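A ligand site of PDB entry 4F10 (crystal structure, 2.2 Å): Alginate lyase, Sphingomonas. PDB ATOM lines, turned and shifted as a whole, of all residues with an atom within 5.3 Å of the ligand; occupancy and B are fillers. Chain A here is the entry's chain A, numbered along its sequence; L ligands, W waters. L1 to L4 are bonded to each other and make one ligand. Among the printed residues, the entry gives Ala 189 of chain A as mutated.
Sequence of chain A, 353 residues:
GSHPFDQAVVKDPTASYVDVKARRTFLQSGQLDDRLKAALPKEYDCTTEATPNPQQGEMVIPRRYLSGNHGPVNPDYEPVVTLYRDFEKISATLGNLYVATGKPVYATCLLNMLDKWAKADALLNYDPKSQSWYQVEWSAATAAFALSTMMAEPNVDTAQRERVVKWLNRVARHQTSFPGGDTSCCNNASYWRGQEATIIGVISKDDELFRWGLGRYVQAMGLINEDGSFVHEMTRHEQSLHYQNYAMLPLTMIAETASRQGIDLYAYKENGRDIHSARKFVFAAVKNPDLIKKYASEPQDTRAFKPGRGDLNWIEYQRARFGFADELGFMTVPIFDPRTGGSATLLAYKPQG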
ATOM      1  N   ARG A  64     -22.409   9.324   6.256  1.00  0.00           N
ATOM      2  CA  ARG A  64     -23.243  10.393   6.765  1.00  0.00           C
ATOM      3  C   ARG A  64     -22.463  11.660   7.113  1.00  0.00           C
ATOM      4  O   ARG A  64     -22.864  12.752   6.722  1.00  0.00           O
ATOM      5  CB  ARG A  64     -24.067   9.943   7.969  1.00  0.00           C
ATOM      6  CG  ARG A  64     -24.789  11.078   8.689  1.00  0.00           C
ATOM      7  CD  ARG A  64     -25.870  10.600   9.646  1.00  0.00           C
ATOM      8  NE  ARG A  64     -27.047  11.453   9.577  1.00  0.00           N
ATOM      9  CZ  ARG A  64     -27.182  12.607  10.227  1.00  0.00           C
ATOM     10  NH1 ARG A  64     -26.197  13.040  10.997  1.00  0.00           N
ATOM     11  NH2 ARG A  64     -28.284  13.329  10.119  1.00  0.00           N
ATOM     12  N   TYR A  65     -21.347  11.504   7.805  1.00  0.00           N
ATOM     13  CA  TYR A  65     -20.606  12.667   8.268  1.00  0.00           C
ATOM     14  C   TYR A  65     -19.468  13.041   7.330  1.00  0.00           C
ATOM     15  O   TYR A  65     -18.743  12.181   6.868  1.00  0.00           O
ATOM     16  CB  TYR A  65     -20.057  12.444   9.676  1.00  0.00           C
ATOM     17  CG  TYR A  65     -21.136  12.463  10.736  1.00  0.00           C
ATOM     18  CD1 TYR A  65     -21.545  11.296  11.362  1.00  0.00           C
ATOM     19  CD2 TYR A  65     -21.788  13.634  11.066  1.00  0.00           C
ATOM     20  CE1 TYR A  65     -22.539  11.310  12.317  1.00  0.00           C
ATOM     21  CE2 TYR A  65     -22.791  13.653  12.018  1.00  0.00           C
ATOM     22  CZ  TYR A  65     -23.157  12.493  12.637  1.00  0.00           C
ATOM     23  OH  TYR A  65     -24.157  12.533  13.576  1.00  0.00           O
ATOM     24  N   GLY A  68     -15.100  12.180  10.335  1.00  0.00           N
ATOM     25  CA  GLY A  68     -15.252  11.650  11.673  1.00  0.00           C
ATOM     26  C   GLY A  68     -16.645  11.129  11.931  1.00  0.00           C
ATOM     27  O   GLY A  68     -17.308  10.638  11.012  1.00  0.00           O
ATOM     28  N   ASN A  69     -17.102  11.251  13.170  1.00  0.00           N
ATOM     29  CA  ASN A  69     -18.430  10.790  13.563  1.00  0.00           C
ATOM     30  C   ASN A  69     -19.334  11.882  14.132  1.00  0.00           C
ATOM     31  O   ASN A  69     -20.218  11.616  14.930  1.00  0.00           O
ATOM     32  CB  ASN A  69     -18.339   9.622  14.546  1.00  0.00           C
ATOM     33  CG  ASN A  69     -17.671  10.018  15.858  1.00  0.00           C
ATOM     34  OD1 ASN A  69     -17.502  11.183  16.158  1.00  0.00           O
ATOM     35  ND2 ASN A  69     -17.293   9.019  16.639  1.00  0.00           N
ATOM     36  N   TYR A  77     -25.131  12.526   1.037  1.00  0.00           N
ATOM     37  CA  TYR A  77     -25.796  11.494   1.808  1.00  0.00           C
ATOM     38  C   TYR A  77     -27.310  11.417   1.555  1.00  0.00           C
ATOM     39  O   TYR A  77     -27.806  10.425   1.037  1.00  0.00           O
ATOM     40  CB  TYR A  77     -25.514  11.691   3.290  1.00  0.00           C
ATOM     41  CG  TYR A  77     -26.149  10.694   4.224  1.00  0.00           C
ATOM     42  CD1 TYR A  77     -25.739   9.371   4.258  1.00  0.00           C
ATOM     43  CD2 TYR A  77     -27.153  11.073   5.089  1.00  0.00           C
ATOM     44  CE1 TYR A  77     -26.315   8.454   5.117  1.00  0.00           C
ATOM     45  CE2 TYR A  77     -27.727  10.164   5.954  1.00  0.00           C
ATOM     46  CZ  TYR A  77     -27.315   8.854   5.970  1.00  0.00           C
ATOM     47  OH  TYR A  77     -27.921   7.982   6.848  1.00  0.00           O
ATOM     48  N   ARG A  85     -35.636   5.782   3.103  1.00  0.00           N
ATOM     49  CA  ARG A  85     -36.585   6.494   3.917  1.00  0.00           C
ATOM     50  C   ARG A  85     -38.034   6.397   3.401  1.00  0.00           C
ATOM     51  O   ARG A  85     -38.940   6.290   4.198  1.00  0.00           O
ATOM     52  CB  ARG A  85     -36.118   7.931   4.164  1.00  0.00           C
ATOM     53  CG  ARG A  85     -34.920   7.964   5.102  1.00  0.00           C
ATOM     54  CD  ARG A  85     -34.215   9.308   5.121  1.00  0.00           C
ATOM     55  NE  ARG A  85     -33.001   9.257   5.928  1.00  0.00           N
ATOM     56  CZ  ARG A  85     -32.388  10.333   6.414  1.00  0.00           C
ATOM     57  NH1 ARG A  85     -32.875  11.538   6.191  1.00  0.00           N
ATOM     58  NH2 ARG A  85     -31.284  10.196   7.135  1.00  0.00           N
ATOM     59  N   GLN A 131     -21.440   2.960   5.045  1.00  0.00           N
ATOM     60  CA  GLN A 131     -22.655   3.493   5.611  1.00  0.00           C
ATOM     61  C   GLN A 131     -23.819   2.516   5.397  1.00  0.00           C
ATOM     62  O   GLN A 131     -24.722   2.436   6.225  1.00  0.00           O
ATOM     63  CB  GLN A 131     -22.982   4.861   5.001  1.00  0.00           C
ATOM     64  CG  GLN A 131     -24.168   5.587   5.606  1.00  0.00           C
ATOM     65  CD  GLN A 131     -24.027   5.834   7.088  1.00  0.00           C
ATOM     66  OE1 GLN A 131     -22.944   6.102   7.586  1.00  0.00           O
ATOM     67  NE2 GLN A 131     -25.132   5.753   7.816  1.00  0.00           N
ATOM     68  N   TYR A 134     -25.211   0.369   8.331  1.00  0.00           N
ATOM     69  CA  TYR A 134     -26.196   0.985   9.199  1.00  0.00           C
ATOM     70  C   TYR A 134     -27.578   1.064   8.563  1.00  0.00           C
ATOM     71  O   TYR A 134     -28.567   0.817   9.219  1.00  0.00           O
ATOM     72  CB  TYR A 134     -25.730   2.366   9.654  1.00  0.00           C
ATOM     73  CG  TYR A 134     -24.417   2.324  10.400  1.00  0.00           C
ATOM     74  CD1 TYR A 134     -24.365   1.930  11.742  1.00  0.00           C
ATOM     75  CD2 TYR A 134     -23.221   2.653   9.786  1.00  0.00           C
ATOM     76  CE1 TYR A 134     -23.163   1.879  12.419  1.00  0.00           C
ATOM     77  CE2 TYR A 134     -22.024   2.597  10.470  1.00  0.00           C
ATOM     78  CZ  TYR A 134     -21.996   2.206  11.783  1.00  0.00           C
ATOM     79  OH  TYR A 134     -20.802   2.159  12.457  1.00  0.00           O
ATOM     80  N   GLN A 135     -27.628   1.430   7.273  1.00  0.00           N
ATOM     81  CA  GLN A 135     -28.900   1.546   6.586  1.00  0.00           C
ATOM     82  C   GLN A 135     -29.689   0.236   6.650  1.00  0.00           C
ATOM     83  O   GLN A 135     -30.904   0.250   6.752  1.00  0.00           O
ATOM     84  CB  GLN A 135     -28.722   2.007   5.145  1.00  0.00           C
ATOM     85  CG  GLN A 135     -30.038   2.346   4.450  1.00  0.00           C
ATOM     86  CD  GLN A 135     -30.841   3.392   5.196  1.00  0.00           C
ATOM     87  OE1 GLN A 135     -30.430   4.540   5.302  1.00  0.00           O
ATOM     88  NE2 GLN A 135     -31.976   3.008   5.727  1.00  0.00           N
ATOM     89  N   TRP A 138     -31.610  -0.285   9.983  1.00  0.00           N
ATOM     90  CA  TRP A 138     -32.770   0.598  10.105  1.00  0.00           C
ATOM     91  C   TRP A 138     -33.934   0.127   9.243  1.00  0.00           C
ATOM     92  O   TRP A 138     -35.066   0.094   9.698  1.00  0.00           O
ATOM     93  CB  TRP A 138     -32.413   2.040   9.725  1.00  0.00           C
ATOM     94  CG  TRP A 138     -31.416   2.710  10.616  1.00  0.00           C
ATOM     95  CD1 TRP A 138     -31.259   2.535  11.956  1.00  0.00           C
ATOM     96  CD2 TRP A 138     -30.409   3.663  10.223  1.00  0.00           C
ATOM     97  NE1 TRP A 138     -30.233   3.318  12.421  1.00  0.00           N
ATOM     98  CE2 TRP A 138     -29.687   4.009  11.381  1.00  0.00           C
ATOM     99  CE3 TRP A 138     -30.048   4.242   9.004  1.00  0.00           C
ATOM    100  CZ2 TRP A 138     -28.631   4.928  11.353  1.00  0.00           C
ATOM    101  CZ3 TRP A 138     -28.983   5.141   8.983  1.00  0.00           C
ATOM    102  CH2 TRP A 138     -28.303   5.479  10.148  1.00  0.00           C
ATOM    103  N   ASN A 187     -21.752   0.556  20.881  1.00  0.00           N
ATOM    104  CA  ASN A 187     -22.484   1.804  21.053  1.00  0.00           C
ATOM    105  C   ASN A 187     -23.932   1.679  20.589  1.00  0.00           C
ATOM    106  O   ASN A 187     -24.443   0.575  20.493  1.00  0.00           O
ATOM    107  CB  ASN A 187     -21.787   2.936  20.309  1.00  0.00           C
ATOM    108  CG  ASN A 187     -21.933   2.821  18.806  1.00  0.00           C
ATOM    109  OD1 ASN A 187     -22.299   1.777  18.280  1.00  0.00           O
ATOM    110  ND2 ASN A 187     -21.634   3.902  18.094  1.00  0.00           N
ATOM    111  N   ASN A 188     -24.581   2.806  20.302  1.00  0.00           N
ATOM    112  CA  ASN A 188     -25.978   2.775  19.901  1.00  0.00           C
ATOM    113  C   ASN A 188     -26.221   1.884  18.659  1.00  0.00           C
ATOM    114  O   ASN A 188     -27.274   1.275  18.548  1.00  0.00           O
ATOM    115  CB  ASN A 188     -26.537   4.178  19.676  1.00  0.00           C
ATOM    116  CG  ASN A 188     -26.102   4.784  18.363  1.00  0.00           C
ATOM    117  OD1 ASN A 188     -25.074   5.458  18.279  1.00  0.00           O
ATOM    118  ND2 ASN A 188     -26.887   4.565  17.330  1.00  0.00           N
ATOM    119  N   ALA A 189     -25.256   1.827  17.754  1.00  0.00           N
ATOM    120  CA  ALA A 189     -25.356   0.969  16.590  1.00  0.00           C
ATOM    121  C   ALA A 189     -25.567  -0.488  17.008  1.00  0.00           C
ATOM    122  O   ALA A 189     -26.369  -1.196  16.404  1.00  0.00           O
ATOM    123  CB  ALA A 189     -24.130   1.104  15.681  1.00  0.00           C
ATOM    124  N   ARG A 236     -19.384  11.876  21.522  1.00  0.00           N
ATOM    125  CA  ARG A 236     -19.824  12.352  20.217  1.00  0.00           C
ATOM    126  C   ARG A 236     -19.855  13.875  20.130  1.00  0.00           C
ATOM    127  O   ARG A 236     -20.464  14.425  19.223  1.00  0.00           O
ATOM    128  CB  ARG A 236     -21.181  11.750  19.845  1.00  0.00           C
ATOM    129  CG  ARG A 236     -21.281  10.225  19.962  1.00  0.00           C
ATOM    130  CD  ARG A 236     -20.345   9.488  19.017  1.00  0.00           C
ATOM    131  NE  ARG A 236     -20.608   9.748  17.600  1.00  0.00           N
ATOM    132  CZ  ARG A 236     -21.432   9.041  16.833  1.00  0.00           C
ATOM    133  NH1 ARG A 236     -22.091   8.014  17.342  1.00  0.00           N
ATOM    134  NH2 ARG A 236     -21.597   9.360  15.559  1.00  0.00           N
ATOM    135  N   HIS A 242     -27.754  14.127  21.885  1.00  0.00           N
ATOM    136  CA  HIS A 242     -28.511  13.508  20.812  1.00  0.00           C
ATOM    137  C   HIS A 242     -28.383  11.991  20.808  1.00  0.00           C
ATOM    138  O   HIS A 242     -29.388  11.287  20.755  1.00  0.00           O
ATOM    139  CB  HIS A 242     -28.077  14.060  19.453  1.00  0.00           C
ATOM    140  CG  HIS A 242     -28.783  13.443  18.309  1.00  0.00           C
ATOM    141  ND1 HIS A 242     -30.018  13.880  17.861  1.00  0.00           N
ATOM    142  CD2 HIS A 242     -28.464  12.393  17.510  1.00  0.00           C
ATOM    143  CE1 HIS A 242     -30.408  13.145  16.852  1.00  0.00           C
ATOM    144  NE2 HIS A 242     -29.482  12.227  16.603  1.00  0.00           N
ATOM    145  N   TYR A 243     -27.158  11.489  20.873  1.00  0.00           N
ATOM    146  CA  TYR A 243     -26.927  10.049  20.768  1.00  0.00           C
ATOM    147  C   TYR A 243     -27.272   9.294  22.044  1.00  0.00           C
ATOM    148  O   TYR A 243     -27.560   8.107  21.999  1.00  0.00           O
ATOM    149  CB  TYR A 243     -25.497   9.741  20.306  1.00  0.00           C
ATOM    150  CG  TYR A 243     -25.306   9.874  18.804  1.00  0.00           C
ATOM    151  CD1 TYR A 243     -24.448  10.831  18.270  1.00  0.00           C
ATOM    152  CD2 TYR A 243     -26.006   9.072  17.919  1.00  0.00           C
ATOM    153  CE1 TYR A 243     -24.294  10.970  16.907  1.00  0.00           C
ATOM    154  CE2 TYR A 243     -25.844   9.206  16.559  1.00  0.00           C
ATOM    155  CZ  TYR A 243     -24.996  10.154  16.040  1.00  0.00           C
ATOM    156  OH  TYR A 243     -24.844  10.285  14.671  1.00  0.00           O
ATOM    157  N   TYR A 246     -30.780   8.871  21.347  1.00  0.00           N
ATOM    158  CA  TYR A 246     -30.861   7.981  20.218  1.00  0.00           C
ATOM    159  C   TYR A 246     -30.720   6.518  20.645  1.00  0.00           C
ATOM    160  O   TYR A 246     -31.376   5.648  20.088  1.00  0.00           O
ATOM    161  CB  TYR A 246     -29.783   8.348  19.207  1.00  0.00           C
ATOM    162  CG  TYR A 246     -30.046   7.901  17.793  1.00  0.00           C
ATOM    163  CD1 TYR A 246     -29.154   7.076  17.130  1.00  0.00           C
ATOM    164  CD2 TYR A 246     -31.184   8.294  17.118  1.00  0.00           C
ATOM    165  CE1 TYR A 246     -29.394   6.663  15.833  1.00  0.00           C
ATOM    166  CE2 TYR A 246     -31.422   7.888  15.827  1.00  0.00           C
ATOM    167  CZ  TYR A 246     -30.525   7.063  15.180  1.00  0.00           C
ATOM    168  OH  TYR A 246     -30.770   6.669  13.891  1.00  0.00           O
ATOM    169  N   ARG A 303     -31.801  19.316  18.373  1.00  0.00           N
ATOM    170  CA  ARG A 303     -32.841  19.242  17.370  1.00  0.00           C
ATOM    171  C   ARG A 303     -33.826  18.103  17.629  1.00  0.00           C
ATOM    172  O   ARG A 303     -34.963  18.164  17.205  1.00  0.00           O
ATOM    173  CB  ARG A 303     -32.233  19.095  15.978  1.00  0.00           C
ATOM    174  CG  ARG A 303     -31.658  17.719  15.689  1.00  0.00           C
ATOM    175  CD  ARG A 303     -30.754  17.734  14.474  1.00  0.00           C
ATOM    176  NE  ARG A 303     -30.417  16.403  14.022  1.00  0.00           N
ATOM    177  CZ  ARG A 303     -29.350  15.729  14.416  1.00  0.00           C
ATOM    178  NH1 ARG A 303     -28.502  16.262  15.285  1.00  0.00           N
ATOM    179  NH2 ARG A 303     -29.123  14.508  13.939  1.00  0.00           N
ATOM    180  N   GLY A 308     -43.039  16.333  18.387  1.00  0.00           N
ATOM    181  CA  GLY A 308     -43.260  15.782  17.063  1.00  0.00           C
ATOM    182  C   GLY A 308     -42.053  15.087  16.477  1.00  0.00           C
ATOM    183  O   GLY A 308     -42.151  14.464  15.424  1.00  0.00           O
ATOM    184  N   ARG A 309     -40.914  15.193  17.135  1.00  0.00           N
ATOM    185  CA  ARG A 309     -39.726  14.536  16.625  1.00  0.00           C
ATOM    186  C   ARG A 309     -39.836  13.016  16.806  1.00  0.00           C
ATOM    187  O   ARG A 309     -40.251  12.546  17.849  1.00  0.00           O
ATOM    188  CB  ARG A 309     -38.467  15.076  17.297  1.00  0.00           C
ATOM    189  CG  ARG A 309     -38.023  16.425  16.774  1.00  0.00           C
ATOM    190  CD  ARG A 309     -37.550  16.342  15.326  1.00  0.00           C
ATOM    191  NE  ARG A 309     -36.374  15.497  15.184  1.00  0.00           N
ATOM    192  CZ  ARG A 309     -35.375  15.709  14.351  1.00  0.00           C
ATOM    193  NH1 ARG A 309     -35.379  16.767  13.552  1.00  0.00           N
ATOM    194  NH2 ARG A 309     -34.361  14.872  14.304  1.00  0.00           N
ATOM    195  N   GLY A 310     -39.511  12.270  15.757  1.00  0.00           N
ATOM    196  CA  GLY A 310     -39.482  10.821  15.832  1.00  0.00           C
ATOM    197  C   GLY A 310     -38.614  10.337  16.969  1.00  0.00           C
ATOM    198  O   GLY A 310     -38.902   9.311  17.572  1.00  0.00           O
ATOM    199  N   ASP A 311     -37.550  11.084  17.249  1.00  0.00           N
ATOM    200  CA  ASP A 311     -36.568  10.734  18.274  1.00  0.00           C
ATOM    201  C   ASP A 311     -37.184  10.480  19.656  1.00  0.00           C
ATOM    202  O   ASP A 311     -36.551   9.868  20.502  1.00  0.00           O
ATOM    203  CB  ASP A 311     -35.497  11.817  18.379  1.00  0.00           C
ATOM    204  CG  ASP A 311     -34.836  12.116  17.041  1.00  0.00           C
ATOM    205  OD1 ASP A 311     -35.482  12.753  16.200  1.00  0.00           O
ATOM    206  OD2 ASP A 311     -33.669  11.732  16.852  1.00  0.00           O
ATOM    207  N   PHE A 336     -44.223   9.946  15.383  1.00  0.00           N
ATOM    208  CA  PHE A 336     -44.151   8.907  14.366  1.00  0.00           C
ATOM    209  C   PHE A 336     -42.702   8.612  14.032  1.00  0.00           C
ATOM    210  O   PHE A 336     -41.957   9.515  13.658  1.00  0.00           O
ATOM    211  CB  PHE A 336     -44.909   9.361  13.112  1.00  0.00           C
ATOM    212  CG  PHE A 336     -44.924   8.346  12.008  1.00  0.00           C
ATOM    213  CD1 PHE A 336     -44.086   8.471  10.906  1.00  0.00           C
ATOM    214  CD2 PHE A 336     -45.780   7.269  12.042  1.00  0.00           C
ATOM    215  CE1 PHE A 336     -44.111   7.537   9.884  1.00  0.00           C
ATOM    216  CE2 PHE A 336     -45.812   6.348  11.022  1.00  0.00           C
ATOM    217  CZ  PHE A 336     -44.980   6.480   9.947  1.00  0.00           C
ATOM    218  N   ARG A 339     -38.747   3.554  12.314  1.00  0.00           N
ATOM    219  CA  ARG A 339     -37.676   2.718  12.818  1.00  0.00           C
ATOM    220  C   ARG A 339     -37.956   2.136  14.199  1.00  0.00           C
ATOM    221  O   ARG A 339     -37.318   1.162  14.608  1.00  0.00           O
ATOM    222  CB  ARG A 339     -36.347   3.502  12.792  1.00  0.00           C
ATOM    223  CG  ARG A 339     -35.827   3.694  11.388  1.00  0.00           C
ATOM    224  CD  ARG A 339     -34.820   4.818  11.243  1.00  0.00           C
ATOM    225  NE  ARG A 339     -34.471   5.002   9.839  1.00  0.00           N
ATOM    226  CZ  ARG A 339     -33.432   5.691   9.395  1.00  0.00           C
ATOM    227  NH1 ARG A 339     -32.590   6.266  10.244  1.00  0.00           N
ATOM    228  NH2 ARG A 339     -33.204   5.795   8.103  1.00  0.00           N
HETATM  229  C1  LIG L   1     -22.208   7.341  11.947  1.00  0.00           C
HETATM  230  C2  LIG L   1     -23.336   7.236  10.878  1.00  0.00           C
HETATM  231  O1  LIG L   1     -23.696   5.858  10.687  1.00  0.00           O
HETATM  232  C3  LIG L   1     -24.565   7.976  11.395  1.00  0.00           C
HETATM  233  O2  LIG L   1     -25.536   7.482  10.464  1.00  0.00           O
HETATM  234  C4  LIG L   1     -25.115   7.435  12.695  1.00  0.00           C
HETATM  235  O3  LIG L   1     -26.353   8.128  13.326  1.00  0.00           O
HETATM  236  C5  LIG L   1     -23.954   7.235  13.715  1.00  0.00           C
HETATM  237  O4  LIG L   1     -22.762   6.705  13.120  1.00  0.00           O
HETATM  238  C6  LIG L   1     -24.321   6.335  14.903  1.00  0.00           C
HETATM  239  O5  LIG L   1     -23.434   6.075  15.740  1.00  0.00           O
HETATM  240  O6  LIG L   1     -25.443   5.790  14.849  1.00  0.00           O
HETATM  241  O7  LIG L   1     -20.902   6.866  11.544  1.00  0.00           O
HETATM  242  C1  LG2 L   2     -27.701   8.436  12.834  1.00  0.00           C
HETATM  243  C2  LG2 L   2     -28.225   9.762  13.491  1.00  0.00           C
HETATM  244  O1  LG2 L   2     -27.518  10.901  12.987  1.00  0.00           O
HETATM  245  C3  LG2 L   2     -29.728   9.879  13.266  1.00  0.00           C
HETATM  246  O2  LG2 L   2     -30.163  11.109  13.835  1.00  0.00           O
HETATM  247  C4  LG2 L   2     -30.031   9.883  11.779  1.00  0.00           C
HETATM  248  O3  LG2 L   2     -31.498   9.996  11.548  1.00  0.00           O
HETATM  249  C5  LG2 L   2     -29.414   8.603  11.131  1.00  0.00           C
HETATM  250  O4  LG2 L   2     -27.992   8.481  11.406  1.00  0.00           O
HETATM  251  C6  LG2 L   2     -29.621   8.614   9.619  1.00  0.00           C
HETATM  252  O5  LG2 L   2     -30.595   7.984   9.173  1.00  0.00           O
HETATM  253  O6  LG2 L   2     -28.712   9.155   8.958  1.00  0.00           O
HETATM  254  C1  LG3 L   3     -31.904  10.731  10.364  1.00  0.00           C
HETATM  255  C2  LG3 L   3     -33.371  10.390  10.057  1.00  0.00           C
HETATM  256  O1  LG3 L   3     -33.455   8.984  10.012  1.00  0.00           O
HETATM  257  C3  LG3 L   3     -34.260  10.893  11.209  1.00  0.00           C
HETATM  258  O2  LG3 L   3     -33.970  10.153  12.404  1.00  0.00           O
HETATM  259  C4  LG3 L   3     -34.088  12.415  11.342  1.00  0.00           C
HETATM  260  O3  LG3 L   3     -34.514  13.023  10.096  1.00  0.00           O
HETATM  261  C5  LG3 L   3     -32.587  12.658  11.548  1.00  0.00           C
HETATM  262  O4  LG3 L   3     -31.779  12.139  10.493  1.00  0.00           O
HETATM  263  C6  LG3 L   3     -32.336  14.146  11.581  1.00  0.00           C
HETATM  264  O5  LG3 L   3     -32.360  14.757  12.623  1.00  0.00           O
HETATM  265  O6  LG3 L   3     -32.048  14.681  10.528  1.00  0.00           O
HETATM  266  C1  LG4 L   4     -35.479  14.064  10.499  1.00  0.00           C
HETATM  267  C2  LG4 L   4     -36.067  14.865   9.323  1.00  0.00           C
HETATM  268  O1  LG4 L   4     -36.914  14.007   8.560  1.00  0.00           O
HETATM  269  C3  LG4 L   4     -36.900  15.997   9.950  1.00  0.00           C
HETATM  270  O2  LG4 L   4     -37.574  16.718   8.924  1.00  0.00           O
HETATM  271  C4  LG4 L   4     -37.897  15.549  10.822  1.00  0.00           C
HETATM  272  C5  LG4 L   4     -37.751  14.376  11.556  1.00  0.00           C
HETATM  273  O3  LG4 L   4     -36.574  13.591  11.436  1.00  0.00           O
HETATM  274  C6  LG4 L   4     -38.737  13.992  12.459  1.00  0.00           C
HETATM  275  O4  LG4 L   4     -38.671  12.951  13.148  1.00  0.00           O
HETATM  276  O5  LG4 L   4     -39.764  14.707  12.587  1.00  0.00           O
HETATM  277  O   HOH W   1     -36.602  11.110  13.308  1.00  0.00           O
HETATM  278  O   HOH W   2     -32.664  11.509  14.449  1.00  0.00           O
HETATM  279  O   HOH W   3     -33.396   7.554  12.882  1.00  0.00           O
HETATM  280  O   HOH W   4     -21.260   4.025  15.094  1.00  0.00           O
HETATM  281  O   HOH W   5     -41.509  12.186  12.120  1.00  0.00           O
HETATM  282  O   HOH W   6     -32.978  14.129   8.027  1.00  0.00           O
HETATM  283  O   HOH W   7     -27.089  13.238  14.759  1.00  0.00           O
HETATM  284  O   HOH W   8     -36.261   7.872  10.542  1.00  0.00           O
HETATM  285  O   HOH W   9     -33.271  17.362  11.457  1.00  0.00           O
HETATM  286  O   HOH W  10     -20.528   8.887   8.914  1.00  0.00           O
HETATM  287  O   HOH W  11     -30.178  13.065   7.864  1.00  0.00           O
HETATM  288  O   HOH W  12     -31.244   6.873   6.620  1.00  0.00           O
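OH of Tyr 65 touches O1 of LG2 L2, at 3.8 Å. CD2 of Tyr 134 touches O1 of LIG L1, 3.4 Å away. Trp 138 touches the ligand. Asn 187 touches the ligand. Tyr 246 touches the ligand. Gly 308 touches the ligand. The nearest printed residue that does not touch the ligand is Asp 311 (4.4 Å).
OD1 of Asp 311 lies within salt-bridge range of NH2 of Arg 309 (3.1 Å). The side-chain hydroxyl (OH) of Tyr 243 lies close to the guanidinium group (NH2) of Arg 236 (3.5 Å). The backbone carbonyl oxygen (O) of Asn 69 lies within hydrogen-bond range of the guanidinium group (NH2) of Arg 236 (2.7 Å). NH1 of Arg 64 lies within hydrogen-bond range of OH of Tyr 65, at 3.3 Å. The side-chain hydroxyl of Tyr 65 lies within hydrogen-bond range of the side-chain hydroxyl of Tyr 243. The backbone NH (N) of Ala 189 lies within hydrogen-bond range of the side-chain amide oxygen (OD1) of Asn 187 (3.0 Å).
An oxygen (O6) of LG2 L2 sits at hydrogen-bond distance from the side-chain hydroxyl (OH) of Tyr 77 (2.5 Å). The guanidinium group (NH2) of Arg 309 lies within salt-bridge range of an oxygen (O5) of LG3 L3, at 2.6 Å. The backbone NH of Gly 310 sits at hydrogen-bond distance from an oxygen (O4) of LG4 L4 (2.8 Å). An oxygen (O5) of LG2 L2 lies within salt-bridge range of the guanidinium group of Arg 339, at 2.8 Å. NH1 of Arg 236 lies within salt-bridge range of O5 of LIG L1, 2.9 Å away. The guanidinium group (NE) of Arg 64 is in salt-bridge range of an oxygen (O6) of LG2 L2, at 2.9 Å. O5 of LG3 L3 lies within salt-bridge range of NE of Arg 303, 2.9 Å away. O3 of LIG L1 sits at hydrogen-bond distance from OH of Tyr 243 (3.0 Å). An oxygen (O2) of LG2 L2 lies within hydrogen-bond range of a ring nitrogen (NE2) of His 242 (3.1 Å). OD1 of Asn 188 lies close to O5 of LIG L1 (3.1 Å). O5 of LG2 L2 is in salt-bridge range of NH2 of Arg 85, at 3.1 Å. An oxygen (O2) of LIG L1 is in hydrogen-bond range of the side-chain amide nitrogen (NE2) of Gln 131 (3.2 Å).
Water W2 lies within hydrogen-bond range of an oxygen (O2) of LG2 L2 (2.6 Å) and the side-chain carboxylate of Asp 311 (2.6 Å). Water W6 bridges O6 of LG3 L3 (2.7 Å) and NH1 of Arg 85 (3.2 Å). Water W9 bridges O5 of LG3 L3 (3.0 Å) and NH1 of Arg 309 (3.0 Å). Water W4 lies within hydrogen-bond range of the side-chain amide nitrogen (ND2) of Asn 187, an oxygen (O5) of LIG L1 and the side-chain hydroxyl (OH) of Tyr 134. Water W5 bridges O5 of LG4 L4 (3.1 Å) and O of Phe 336 (3.1 Å). Water W10 lies within hydrogen-bond range of the backbone NH of Tyr 65 (3.0 Å), the backbone NH of Arg 64 (3.3 Å) and an oxygen (O7) of LIG L1 (3.3 Å).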
